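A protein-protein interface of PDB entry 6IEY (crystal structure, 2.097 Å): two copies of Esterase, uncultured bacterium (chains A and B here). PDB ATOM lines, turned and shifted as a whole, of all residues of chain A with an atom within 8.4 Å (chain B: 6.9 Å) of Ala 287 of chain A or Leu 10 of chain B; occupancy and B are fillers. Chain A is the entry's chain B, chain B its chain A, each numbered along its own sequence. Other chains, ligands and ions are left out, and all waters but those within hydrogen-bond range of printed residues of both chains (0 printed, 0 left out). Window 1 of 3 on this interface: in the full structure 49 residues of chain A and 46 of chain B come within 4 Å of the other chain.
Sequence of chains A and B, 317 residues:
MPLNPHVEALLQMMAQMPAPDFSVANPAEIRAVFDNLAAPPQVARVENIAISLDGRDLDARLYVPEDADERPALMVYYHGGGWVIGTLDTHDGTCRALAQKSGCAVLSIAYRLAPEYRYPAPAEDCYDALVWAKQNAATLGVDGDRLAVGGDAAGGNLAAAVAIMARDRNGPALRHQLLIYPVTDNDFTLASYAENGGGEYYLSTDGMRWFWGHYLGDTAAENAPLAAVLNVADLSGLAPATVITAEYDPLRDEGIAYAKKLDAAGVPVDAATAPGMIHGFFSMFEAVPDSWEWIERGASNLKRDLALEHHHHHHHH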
ATOM      1  N   ALA A   9      -1.915  -9.858   9.748  1.00  0.00           N
ATOM      2  CA  ALA A   9      -2.873  -8.756   9.850  1.00  0.00           C
ATOM      3  C   ALA A   9      -3.170  -8.412  11.317  1.00  0.00           C
ATOM      4  O   ALA A   9      -3.420  -7.251  11.664  1.00  0.00           O
ATOM      5  CB  ALA A   9      -4.156  -9.097   9.122  1.00  0.00           C
ATOM      6  N   LEU A  10      -3.146  -9.424  12.178  1.00  0.00           N
ATOM      7  CA  LEU A  10      -3.350  -9.190  13.598  1.00  0.00           C
ATOM      8  C   LEU A  10      -2.169  -8.411  14.169  1.00  0.00           C
ATOM      9  O   LEU A  10      -2.357  -7.440  14.884  1.00  0.00           O
ATOM     10  CB  LEU A  10      -3.543 -10.510  14.346  1.00  0.00           C
ATOM     11  CG  LEU A  10      -3.841 -10.364  15.835  1.00  0.00           C
ATOM     12  CD1 LEU A  10      -4.980  -9.397  16.054  1.00  0.00           C
ATOM     13  CD2 LEU A  10      -4.160 -11.724  16.450  1.00  0.00           C
ATOM     14  N   MET A  13      -2.283  -4.883  13.178  1.00  0.00           N
ATOM     15  CA  MET A  13      -3.340  -4.165  13.877  1.00  0.00           C
ATOM     16  C   MET A  13      -2.967  -3.864  15.329  1.00  0.00           C
ATOM     17  O   MET A  13      -3.278  -2.791  15.832  1.00  0.00           O
ATOM     18  CB  MET A  13      -4.650  -4.949  13.824  1.00  0.00           C
ATOM     19  CG  MET A  13      -5.785  -4.266  14.582  1.00  0.00           C
ATOM     20  SD  MET A  13      -7.418  -4.855  14.102  1.00  0.00           S
ATOM     21  CE  MET A  13      -7.536  -4.178  12.452  1.00  0.00           C
ATOM     22  N   MET A  14      -2.309  -4.805  16.000  1.00  0.00           N
ATOM     23  CA  MET A  14      -1.829  -4.566  17.355  1.00  0.00           C
ATOM     24  C   MET A  14      -0.813  -3.429  17.367  1.00  0.00           C
ATOM     25  O   MET A  14      -0.724  -2.679  18.339  1.00  0.00           O
ATOM     26  CB  MET A  14      -1.204  -5.830  17.954  1.00  0.00           C
ATOM     27  CG  MET A  14      -2.185  -6.752  18.667  1.00  0.00           C
ATOM     28  SD  MET A  14      -1.496  -8.404  18.999  1.00  0.00           S
ATOM     29  CE  MET A  14      -0.110  -8.007  20.070  1.00  0.00           C
ATOM     30  N   GLN A  16      -0.694  -0.772  15.459  1.00  0.00           N
ATOM     31  CA  GLN A  16      -1.286   0.540  15.222  1.00  0.00           C
ATOM     32  C   GLN A  16      -2.177   0.934  16.380  1.00  0.00           C
ATOM     33  O   GLN A  16      -3.061   1.773  16.238  1.00  0.00           O
ATOM     34  CB  GLN A  16      -2.081   0.545  13.922  1.00  0.00           C
ATOM     35  CG  GLN A  16      -1.235   0.293  12.700  1.00  0.00           C
ATOM     36  CD  GLN A  16      -2.064   0.064  11.445  1.00  0.00           C
ATOM     37  OE1 GLN A  16      -3.263   0.362  11.411  1.00  0.00           O
ATOM     38  NE2 GLN A  16      -1.430  -0.483  10.406  1.00  0.00           N
ATOM     39  N   MET A  17      -1.947   0.319  17.530  1.00  0.00           N
ATOM     40  CA  MET A  17      -2.758   0.594  18.702  1.00  0.00           C
ATOM     41  C   MET A  17      -2.084   1.639  19.589  1.00  0.00           C
ATOM     42  O   MET A  17      -0.853   1.723  19.627  1.00  0.00           O
ATOM     43  CB  MET A  17      -3.015  -0.698  19.482  1.00  0.00           C
ATOM     44  CG  MET A  17      -4.007  -1.624  18.800  1.00  0.00           C
ATOM     45  SD  MET A  17      -5.572  -0.793  18.443  1.00  0.00           S
ATOM     46  CE  MET A  17      -5.918  -1.448  16.810  1.00  0.00           C
ATOM     47  N   PRO A  18      -2.896   2.453  20.290  1.00  0.00           N
ATOM     48  CA  PRO A  18      -2.403   3.457  21.241  1.00  0.00           C
ATOM     49  C   PRO A  18      -1.401   2.879  22.234  1.00  0.00           C
ATOM     50  O   PRO A  18      -1.773   2.009  23.027  1.00  0.00           O
ATOM     51  CB  PRO A  18      -3.678   3.911  21.965  1.00  0.00           C
ATOM     52  CG  PRO A  18      -4.762   3.706  20.977  1.00  0.00           C
ATOM     53  CD  PRO A  18      -4.367   2.484  20.173  1.00  0.00           C
ATOM     54  N   LEU A  37      -5.280  -5.729  26.881  1.00  0.00           N
ATOM     55  CA  LEU A  37      -5.217  -6.344  25.563  1.00  0.00           C
ATOM     56  C   LEU A  37      -6.120  -7.564  25.433  1.00  0.00           C
ATOM     57  O   LEU A  37      -6.786  -7.735  24.417  1.00  0.00           O
ATOM     58  CB  LEU A  37      -3.775  -6.750  25.233  1.00  0.00           C
ATOM     59  CG  LEU A  37      -3.581  -7.532  23.925  1.00  0.00           C
ATOM     60  CD1 LEU A  37      -3.677  -6.585  22.728  1.00  0.00           C
ATOM     61  CD2 LEU A  37      -2.268  -8.329  23.901  1.00  0.00           C
ATOM     62  N   GLU A 200     -19.850  -3.008   1.724  1.00  0.00           N
ATOM     63  CA  GLU A 200     -18.572  -2.370   2.003  1.00  0.00           C
ATOM     64  C   GLU A 200     -18.383  -2.055   3.489  1.00  0.00           C
ATOM     65  O   GLU A 200     -17.258  -2.062   3.997  1.00  0.00           O
ATOM     66  CB  GLU A 200     -18.505  -1.083   1.182  1.00  0.00           C
ATOM     67  CG  GLU A 200     -19.957  -0.701   0.816  1.00  0.00           C
ATOM     68  CD  GLU A 200     -20.134   0.727   0.487  1.00  0.00           C
ATOM     69  OE1 GLU A 200     -19.174   1.475   0.713  1.00  0.00           O
ATOM     70  OE2 GLU A 200     -21.240   1.116   0.035  1.00  0.00           O
ATOM     71  N   TYR A 202     -19.806  -3.636   6.290  1.00  0.00           N
ATOM     72  CA  TYR A 202     -20.318  -4.697   7.166  1.00  0.00           C
ATOM     73  C   TYR A 202     -21.811  -4.946   6.911  1.00  0.00           C
ATOM     74  O   TYR A 202     -22.180  -5.835   6.136  1.00  0.00           O
ATOM     75  CB  TYR A 202     -20.045  -4.325   8.633  1.00  0.00           C
ATOM     76  CG  TYR A 202     -20.561  -5.279   9.688  1.00  0.00           C
ATOM     77  CD1 TYR A 202     -20.347  -6.654   9.588  1.00  0.00           C
ATOM     78  CD2 TYR A 202     -21.231  -4.791  10.818  1.00  0.00           C
ATOM     79  CE1 TYR A 202     -20.813  -7.523  10.569  1.00  0.00           C
ATOM     80  CE2 TYR A 202     -21.694  -5.653  11.815  1.00  0.00           C
ATOM     81  CZ  TYR A 202     -21.485  -7.019  11.681  1.00  0.00           C
ATOM     82  OH  TYR A 202     -21.946  -7.877  12.666  1.00  0.00           O
ATOM     83  N   ILE A 278     -18.685   2.875  11.375  1.00  0.00           N
ATOM     84  CA  ILE A 278     -19.625   2.014  10.680  1.00  0.00           C
ATOM     85  C   ILE A 278     -20.641   1.408  11.652  1.00  0.00           C
ATOM     86  O   ILE A 278     -20.482   1.496  12.876  1.00  0.00           O
ATOM     87  CB  ILE A 278     -18.926   0.855   9.933  1.00  0.00           C
ATOM     88  CG1 ILE A 278     -18.171  -0.052  10.908  1.00  0.00           C
ATOM     89  CG2 ILE A 278     -18.016   1.390   8.833  1.00  0.00           C
ATOM     90  CD1 ILE A 278     -17.587  -1.274  10.257  1.00  0.00           C
ATOM     91  N   HIS A 279     -21.676   0.784  11.101  1.00  0.00           N
ATOM     92  CA  HIS A 279     -22.601  -0.005  11.910  1.00  0.00           C
ATOM     93  C   HIS A 279     -21.878  -0.996  12.819  1.00  0.00           C
ATOM     94  O   HIS A 279     -20.985  -1.700  12.371  1.00  0.00           O
ATOM     95  CB  HIS A 279     -23.558  -0.784  11.034  1.00  0.00           C
ATOM     96  CG  HIS A 279     -24.710  -1.357  11.793  1.00  0.00           C
ATOM     97  ND1 HIS A 279     -25.756  -0.584  12.244  1.00  0.00           N
ATOM     98  CD2 HIS A 279     -24.958  -2.617  12.217  1.00  0.00           C
ATOM     99  CE1 HIS A 279     -26.619  -1.349  12.886  1.00  0.00           C
ATOM    100  NE2 HIS A 279     -26.162  -2.588  12.880  1.00  0.00           N
ATOM    101  N   GLY A 280     -22.275  -1.058  14.088  1.00  0.00           N
ATOM    102  CA  GLY A 280     -21.723  -2.056  14.980  1.00  0.00           C
ATOM    103  C   GLY A 280     -20.512  -1.581  15.741  1.00  0.00           C
ATOM    104  O   GLY A 280     -19.877  -2.361  16.455  1.00  0.00           O
ATOM    105  N   PHE A 281     -20.184  -0.299  15.634  1.00  0.00           N
ATOM    106  CA  PHE A 281     -18.888   0.132  16.158  1.00  0.00           C
ATOM    107  C   PHE A 281     -18.813   0.225  17.691  1.00  0.00           C
ATOM    108  O   PHE A 281     -17.708   0.319  18.237  1.00  0.00           O
ATOM    109  CB  PHE A 281     -18.471   1.468  15.540  1.00  0.00           C
ATOM    110  CG  PHE A 281     -19.131   2.671  16.143  1.00  0.00           C
ATOM    111  CD1 PHE A 281     -20.344   3.129  15.658  1.00  0.00           C
ATOM    112  CD2 PHE A 281     -18.497   3.398  17.148  1.00  0.00           C
ATOM    113  CE1 PHE A 281     -20.932   4.264  16.184  1.00  0.00           C
ATOM    114  CE2 PHE A 281     -19.092   4.536  17.687  1.00  0.00           C
ATOM    115  CZ  PHE A 281     -20.309   4.971  17.193  1.00  0.00           C
ATOM    116  N   SER A 283     -19.456  -2.261  19.483  1.00  0.00           N
ATOM    117  CA  SER A 283     -18.912  -3.577  19.783  1.00  0.00           C
ATOM    118  C   SER A 283     -17.474  -3.729  19.301  1.00  0.00           C
ATOM    119  O   SER A 283     -16.862  -4.760  19.550  1.00  0.00           O
ATOM    120  CB  SER A 283     -19.760  -4.693  19.147  1.00  0.00           C
ATOM    121  OG  SER A 283     -21.140  -4.494  19.351  1.00  0.00           O
ATOM    122  N   MET A 284     -16.937  -2.721  18.609  1.00  0.00           N
ATOM    123  CA  MET A 284     -15.594  -2.836  18.029  1.00  0.00           C
ATOM    124  C   MET A 284     -14.490  -2.084  18.768  1.00  0.00           C
ATOM    125  O   MET A 284     -13.414  -1.864  18.209  1.00  0.00           O
ATOM    126  CB  MET A 284     -15.600  -2.348  16.581  1.00  0.00           C
ATOM    127  CG  MET A 284     -16.580  -3.060  15.708  1.00  0.00           C
ATOM    128  SD  MET A 284     -16.867  -2.174  14.160  1.00  0.00           S
ATOM    129  CE  MET A 284     -18.185  -3.185  13.484  1.00  0.00           C
ATOM    130  N   PHE A 285     -14.742  -1.715  20.020  1.00  0.00           N
ATOM    131  CA  PHE A 285     -13.804  -0.918  20.800  1.00  0.00           C
ATOM    132  C   PHE A 285     -12.416  -1.555  20.980  1.00  0.00           C
ATOM    133  O   PHE A 285     -11.427  -0.854  21.186  1.00  0.00           O
ATOM    134  CB  PHE A 285     -14.419  -0.618  22.171  1.00  0.00           C
ATOM    135  CG  PHE A 285     -14.775  -1.845  22.950  1.00  0.00           C
ATOM    136  CD1 PHE A 285     -13.806  -2.526  23.687  1.00  0.00           C
ATOM    137  CD2 PHE A 285     -16.073  -2.314  22.961  1.00  0.00           C
ATOM    138  CE1 PHE A 285     -14.126  -3.657  24.412  1.00  0.00           C
ATOM    139  CE2 PHE A 285     -16.412  -3.453  23.689  1.00  0.00           C
ATOM    140  CZ  PHE A 285     -15.440  -4.120  24.415  1.00  0.00           C
ATOM    141  N   GLU A 286     -12.326  -2.876  20.906  1.00  0.00           N
ATOM    142  CA  GLU A 286     -11.025  -3.503  21.086  1.00  0.00           C
ATOM    143  C   GLU A 286     -10.092  -3.159  19.930  1.00  0.00           C
ATOM    144  O   GLU A 286      -8.892  -3.033  20.126  1.00  0.00           O
ATOM    145  CB  GLU A 286     -11.153  -5.024  21.230  1.00  0.00           C
ATOM    146  CG  GLU A 286     -11.436  -5.446  22.653  1.00  0.00           C
ATOM    147  CD  GLU A 286     -11.622  -6.947  22.812  1.00  0.00           C
ATOM    148  OE1 GLU A 286     -11.275  -7.692  21.863  1.00  0.00           O
ATOM    149  OE2 GLU A 286     -12.101  -7.376  23.896  1.00  0.00           O
ATOM    150  N   ALA A 287     -10.647  -3.007  18.732  1.00  0.00           N
ATOM    151  CA  ALA A 287      -9.824  -2.750  17.558  1.00  0.00           C
ATOM    152  C   ALA A 287      -9.903  -1.285  17.156  1.00  0.00           C
ATOM    153  O   ALA A 287      -9.014  -0.771  16.481  1.00  0.00           O
ATOM    154  CB  ALA A 287     -10.251  -3.649  16.400  1.00  0.00           C
ATOM    155  N   VAL A 288     -10.986  -0.625  17.563  1.00  0.00           N
ATOM    156  CA  VAL A 288     -11.216   0.765  17.221  1.00  0.00           C
ATOM    157  C   VAL A 288     -11.260   1.609  18.486  1.00  0.00           C
ATOM    158  O   VAL A 288     -12.326   1.823  19.052  1.00  0.00           O
ATOM    159  CB  VAL A 288     -12.528   0.946  16.440  1.00  0.00           C
ATOM    160  CG1 VAL A 288     -12.697   2.413  15.979  1.00  0.00           C
ATOM    161  CG2 VAL A 288     -12.574  -0.026  15.265  1.00  0.00           C
ATOM    162  N   PRO A 289     -10.097   2.113  18.914  1.00  0.00           N
ATOM    163  CA  PRO A 289      -9.973   2.880  20.158  1.00  0.00           C
ATOM    164  C   PRO A 289     -11.004   4.011  20.254  1.00  0.00           C
ATOM    165  O   PRO A 289     -11.528   4.315  21.321  1.00  0.00           O
ATOM    166  CB  PRO A 289      -8.544   3.444  20.080  1.00  0.00           C
ATOM    167  CG  PRO A 289      -7.826   2.545  19.147  1.00  0.00           C
ATOM    168  CD  PRO A 289      -8.845   2.117  18.138  1.00  0.00           C
ATOM    169  N   ASP A 290     -11.317   4.605  19.115  1.00  0.00           N
ATOM    170  CA  ASP A 290     -12.198   5.753  19.074  1.00  0.00           C
ATOM    171  C   ASP A 290     -13.650   5.419  19.457  1.00  0.00           C
ATOM    172  O   ASP A 290     -14.430   6.322  19.793  1.00  0.00           O
ATOM    173  CB  ASP A 290     -12.124   6.376  17.684  1.00  0.00           C
ATOM    174  CG  ASP A 290     -10.682   6.658  17.256  1.00  0.00           C
ATOM    175  OD1 ASP A 290     -10.204   7.773  17.582  1.00  0.00           O
ATOM    176  OD2 ASP A 290     -10.032   5.771  16.621  1.00  0.00           O
ATOM    177  N   SER A 291     -14.001   4.134  19.427  1.00  0.00           N
ATOM    178  CA  SER A 291     -15.326   3.683  19.879  1.00  0.00           C
ATOM    179  C   SER A 291     -15.603   4.077  21.322  1.00  0.00           C
ATOM    180  O   SER A 291     -16.753   4.350  21.686  1.00  0.00           O
ATOM    181  CB  SER A 291     -15.471   2.161  19.754  1.00  0.00           C
ATOM    182  OG  SER A 291     -15.597   1.764  18.400  1.00  0.00           O
ATOM    183  N   TRP A 292     -14.557   4.072  22.145  1.00  0.00           N
ATOM    184  CA  TRP A 292     -14.714   4.378  23.558  1.00  0.00           C
ATOM    185  C   TRP A 292     -15.270   5.788  23.794  1.00  0.00           C
ATOM    186  O   TRP A 292     -16.066   6.003  24.714  1.00  0.00           O
ATOM    187  CB  TRP A 292     -13.386   4.200  24.284  1.00  0.00           C
ATOM    188  CG  TRP A 292     -13.102   2.777  24.664  1.00  0.00           C
ATOM    189  CD1 TRP A 292     -12.142   1.966  24.139  1.00  0.00           C
ATOM    190  CD2 TRP A 292     -13.782   1.995  25.669  1.00  0.00           C
ATOM    191  NE1 TRP A 292     -12.176   0.726  24.753  1.00  0.00           N
ATOM    192  CE2 TRP A 292     -13.171   0.724  25.696  1.00  0.00           C
ATOM    193  CE3 TRP A 292     -14.847   2.250  26.549  1.00  0.00           C
ATOM    194  CZ2 TRP A 292     -13.582  -0.296  26.571  1.00  0.00           C
ATOM    195  CZ3 TRP A 292     -15.264   1.229  27.416  1.00  0.00           C
ATOM    196  CH2 TRP A 292     -14.625  -0.027  27.416  1.00  0.00           C
ATOM    197  N   ASN B   4     -12.785   5.671   9.477  1.00  0.00           N
ATOM    198  CA  ASN B   4     -11.767   5.515  10.504  1.00  0.00           C
ATOM    199  C   ASN B   4     -10.797   4.403  10.099  1.00  0.00           C
ATOM    200  O   ASN B   4     -11.231   3.308   9.756  1.00  0.00           O
ATOM    201  CB  ASN B   4     -12.424   5.228  11.855  1.00  0.00           C
ATOM    202  CG  ASN B   4     -11.415   5.052  12.971  1.00  0.00           C
ATOM    203  OD1 ASN B   4     -10.800   3.998  13.108  1.00  0.00           O
ATOM    204  ND2 ASN B   4     -11.246   6.086  13.779  1.00  0.00           N
ATOM    205  N   PRO B   5      -9.483   4.697  10.096  1.00  0.00           N
ATOM    206  CA  PRO B   5      -8.425   3.761   9.687  1.00  0.00           C
ATOM    207  C   PRO B   5      -8.373   2.470  10.493  1.00  0.00           C
ATOM    208  O   PRO B   5      -7.970   1.440   9.938  1.00  0.00           O
ATOM    209  CB  PRO B   5      -7.140   4.564   9.898  1.00  0.00           C
ATOM    210  CG  PRO B   5      -7.530   5.737  10.754  1.00  0.00           C
ATOM    211  CD  PRO B   5      -8.940   6.035  10.389  1.00  0.00           C
ATOM    212  N   HIS B   6      -8.748   2.514  11.774  1.00  0.00           N
ATOM    213  CA  HIS B   6      -8.841   1.279  12.546  1.00  0.00           C
ATOM    214  C   HIS B   6     -10.043   0.503  12.057  1.00  0.00           C
ATOM    215  O   HIS B   6     -10.025  -0.718  12.007  1.00  0.00           O
ATOM    216  CB  HIS B   6      -8.955   1.548  14.045  1.00  0.00           C
ATOM    217  CG  HIS B   6      -7.733   2.167  14.634  1.00  0.00           C
ATOM    218  ND1 HIS B   6      -7.634   3.519  14.893  1.00  0.00           N
ATOM    219  CD2 HIS B   6      -6.548   1.623  15.000  1.00  0.00           C
ATOM    220  CE1 HIS B   6      -6.444   3.778  15.403  1.00  0.00           C
ATOM    221  NE2 HIS B   6      -5.764   2.646  15.477  1.00  0.00           N
ATOM    222  N   VAL B   7     -11.092   1.228  11.699  1.00  0.00           N
ATOM    223  CA  VAL B   7     -12.288   0.588  11.193  1.00  0.00           C
ATOM    224  C   VAL B   7     -11.972  -0.044   9.833  1.00  0.00           C
ATOM    225  O   VAL B   7     -12.311  -1.195   9.577  1.00  0.00           O
ATOM    226  CB  VAL B   7     -13.436   1.580  11.074  1.00  0.00           C
ATOM    227  CG1 VAL B   7     -14.576   0.963  10.308  1.00  0.00           C
ATOM    228  CG2 VAL B   7     -13.891   2.033  12.462  1.00  0.00           C
ATOM    229  N   GLU B   8     -11.284   0.706   8.977  1.00  0.00           N
ATOM    230  CA  GLU B   8     -10.931   0.202   7.658  1.00  0.00           C
ATOM    231  C   GLU B   8     -10.002  -1.018   7.758  1.00  0.00           C
ATOM    232  O   GLU B   8     -10.169  -1.997   7.027  1.00  0.00           O
ATOM    233  CB  GLU B   8     -10.284   1.313   6.822  1.00  0.00           C
ATOM    234  CG  GLU B   8     -10.459   1.107   5.323  1.00  0.00           C
ATOM    235  CD  GLU B   8      -9.565   1.996   4.491  1.00  0.00           C
ATOM    236  OE1 GLU B   8      -9.207   3.097   4.969  1.00  0.00           O
ATOM    237  OE2 GLU B   8      -9.215   1.589   3.357  1.00  0.00           O
ATOM    238  N   ALA B   9      -9.040  -0.980   8.677  1.00  0.00           N
ATOM    239  CA  ALA B   9      -8.195  -2.152   8.921  1.00  0.00           C
ATOM    240  C   ALA B   9      -9.015  -3.344   9.437  1.00  0.00           C
ATOM    241  O   ALA B   9      -8.748  -4.496   9.091  1.00  0.00           O
ATOM    242  CB  ALA B   9      -7.083  -1.810   9.904  1.00  0.00           C
ATOM    243  N   LEU B  10     -10.012  -3.073  10.271  1.00  0.00           N
ATOM    244  CA  LEU B  10     -10.876  -4.145  10.741  1.00  0.00           C
ATOM    245  C   LEU B  10     -11.686  -4.727   9.581  1.00  0.00           C
ATOM    246  O   LEU B  10     -11.849  -5.945   9.478  1.00  0.00           O
ATOM    247  CB  LEU B  10     -11.808  -3.655  11.849  1.00  0.00           C
ATOM    248  CG  LEU B  10     -12.502  -4.831  12.553  1.00  0.00           C
ATOM    249  CD1 LEU B  10     -11.535  -5.564  13.482  1.00  0.00           C
ATOM    250  CD2 LEU B  10     -13.743  -4.368  13.304  1.00  0.00           C
ATOM    251  N   LEU B  11     -12.173  -3.858   8.696  1.00  0.00           N
ATOM    252  CA  LEU B  11     -13.010  -4.295   7.581  1.00  0.00           C
ATOM    253  C   LEU B  11     -12.252  -5.216   6.636  1.00  0.00           C
ATOM    254  O   LEU B  11     -12.768  -6.257   6.231  1.00  0.00           O
ATOM    255  CB  LEU B  11     -13.562  -3.091   6.813  1.00  0.00           C
ATOM    256  CG  LEU B  11     -14.710  -2.373   7.519  1.00  0.00           C
ATOM    257  CD1 LEU B  11     -15.048  -1.085   6.791  1.00  0.00           C
ATOM    258  CD2 LEU B  11     -15.938  -3.260   7.590  1.00  0.00           C
ATOM    259  N   GLN B  12     -11.026  -4.842   6.293  1.00  0.00           N
ATOM    260  CA  GLN B  12     -10.215  -5.674   5.417  1.00  0.00           C
ATOM    261  C   GLN B  12      -9.794  -6.974   6.116  1.00  0.00           C
ATOM    262  O   GLN B  12      -9.533  -7.987   5.463  1.00  0.00           O
ATOM    263  CB  GLN B  12      -8.989  -4.900   4.925  1.00  0.00           C
ATOM    264  CG  GLN B  12      -9.047  -4.567   3.429  1.00  0.00           C
ATOM    265  CD  GLN B  12      -9.232  -5.818   2.566  1.00  0.00           C
ATOM    266  OE1 GLN B  12     -10.075  -5.850   1.663  1.00  0.00           O
ATOM    267  NE2 GLN B  12      -8.434  -6.852   2.842  1.00  0.00           N
ATOM    268  N   MET B  13      -9.748  -6.951   7.444  1.00  0.00           N
ATOM    269  CA  MET B  13      -9.474  -8.163   8.211  1.00  0.00           C
ATOM    270  C   MET B  13     -10.634  -9.156   8.087  1.00  0.00           C
ATOM    271  O   MET B  13     -10.423 -10.362   7.922  1.00  0.00           O
ATOM    272  CB  MET B  13      -9.217  -7.825   9.679  1.00  0.00           C
ATOM    273  CG  MET B  13      -8.960  -9.031  10.561  1.00  0.00           C
ATOM    274  SD  MET B  13      -8.644  -8.527  12.267  1.00  0.00           S
ATOM    275  CE  MET B  13      -7.061  -7.721  12.081  1.00  0.00           C
ATOM    276  N   MET B  14     -11.858  -8.644   8.163  1.00  0.00           N
ATOM    277  CA  MET B  14     -13.041  -9.474   7.955  1.00  0.00           C
ATOM    278  C   MET B  14     -13.112  -9.992   6.522  1.00  0.00           C
ATOM    279  O   MET B  14     -13.350 -11.178   6.295  1.00  0.00           O
ATOM    280  CB  MET B  14     -14.306  -8.691   8.270  1.00  0.00           C
ATOM    281  CG  MET B  14     -14.355  -8.127   9.665  1.00  0.00           C
ATOM    282  SD  MET B  14     -15.604  -6.839   9.741  1.00  0.00           S
ATOM    283  CE  MET B  14     -16.991  -7.696   8.982  1.00  0.00           C
ATOM    284  N   ALA B  15     -12.908  -9.091   5.561  1.00  0.00           N
ATOM    285  CA  ALA B  15     -12.930  -9.439   4.138  1.00  0.00           C
ATOM    286  C   ALA B  15     -11.907 -10.523   3.819  1.00  0.00           C
ATOM    287  O   ALA B  15     -12.112 -11.355   2.930  1.00  0.00           O
ATOM    288  CB  ALA B  15     -12.675  -8.207   3.290  1.00  0.00           C
ATOM    289  N   GLN B  16     -10.810 -10.510   4.570  1.00  0.00           N
ATOM    290  CA  GLN B  16      -9.723 -11.465   4.411  1.00  0.00           C
ATOM    291  C   GLN B  16     -10.086 -12.856   4.947  1.00  0.00           C
ATOM    292  O   GLN B  16      -9.287 -13.796   4.860  1.00  0.00           O
ATOM    293  CB  GLN B  16      -8.477 -10.937   5.115  1.00  0.00           C
ATOM    294  CG  GLN B  16      -7.170 -11.576   4.696  1.00  0.00           C
ATOM    295  CD  GLN B  16      -6.029 -11.120   5.584  1.00  0.00           C
ATOM    296  OE1 GLN B  16      -6.120 -10.071   6.235  1.00  0.00           O
ATOM    297  NE2 GLN B  16      -4.956 -11.910   5.633  1.00  0.00           N
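The side-chain carboxylate (OD2) of Asp 290 of chain A lies within hydrogen-bond range of the side-chain amide nitrogen (ND2) of Asn 4 of chain B, 3.1 Å away. The backbone carbonyl oxygen of Gln 16 of chain A is in hydrogen-bond range of a ring nitrogen (NE2) of His 6 of chain B, at 2.9 Å.
The side-chain amide oxygen (OD1) of Asn 4 of chain B is in hydrogen-bond range of the backbone NH (N) of Val 7 of chain B, at 3.1 Å. The side-chain amide oxygen of Asn 4 of chain B is in hydrogen-bond range of the backbone NH of His 6 of chain B (2.9 Å). The side-chain hydroxyl (OG) of Ser 291 of chain A sits close to the backbone carbonyl oxygen (O) of Val 288 of chain A (3.3 Å).
Among the printed residues, merely in contact across the chains: Ala 9 of chain A with Met 13 of chain B (3.7 Å), Ala 9 of chain A with Gln 16 of chain B (3.6 Å), Met 13 of chain A with Ala 9 of chain B (3.5 Å), Met 13 of chain A with Leu 10 of chain B (3.5 Å), Met 13 of chain A with Met 13 of chain B (3.5 Å), Met 17 of chain A with His 6 of chain B (3.6 Å), Glu 200 of chain A with Leu 11 of chain B (3.7 Å), Tyr 202 of chain A with Met 14 of chain B (3.6 Å), Ile 278 of chain A with Val 7 of chain B (3.8 Å), Ile 278 of chain A with Leu 11 of chain B (3.7 Å), Met 284 of chain A with Leu 10 of chain B (3.9 Å), Ala 287 of chain A with His 6 of chain B (3.4 Å), Ala 287 of chain A with Leu 10 of chain B (3.7 Å), Val 288 of chain A with Asn 4 of chain B (3.8 Å), Val 288 of chain A with His 6 of chain B (3.98 Å), Val 288 of chain A with Val 7 of chain B (3.7 Å), Pro 289 of chain A with His 6 of chain B (3.7 Å) and Asp 290 of chain A with His 6 of chain B (3.7 Å).
Leu 10 of chain B touches just these residues of chain A: Met 13, Met 284 and Ala 287. Of the printed residues of chain A, Ala 9 of chain B touches Met 13. Of the printed residues of chain B, Ile 278 of chain A touches Val 7 (3.8 Å) and Leu 11 (3.7 Å). Of the printed residues of chain A, Met 14 of chain B touches Tyr 202. Of the printed residues of chain B, Tyr 202 of chain A touches Met 14 (3.6 Å). The nearest printed residue of chain B that does not touch Ile 278 of chain A is Leu 10 of chain B (5.8 Å).
Hydrophobic or aromatic side chains of chain A that line the printed part of chain B: Ala 9, Met 13, Met 17, Tyr 202, Ile 278, Met 284, Ala 287, Val 288 and Pro 289.
Ala 9 of chain A touches Met 13 of chain B, and with the chains exchanged Met 13 of chain A touches Ala 9 of chain B. Ala 9 of chain A touches Gln 16 of chain B, but with the chains exchanged Gln 16 of chain A does not touch Ala 9 of chain B (4.6 Å). Met 13 of chain A touches Leu 10 of chain B, but with the chains exchanged Leu 10 of chain A does not touch Met 13 of chain B (4.3 Å). Met 13 of chain A touches its own counterpart, Met 13 of chain B. Positions printed for both chains: 9, 10, 13, 14 and 16. Of the 20 pairs that touch across the chains among the printed residues, 3 have their exchanged pair printed and touching as well.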
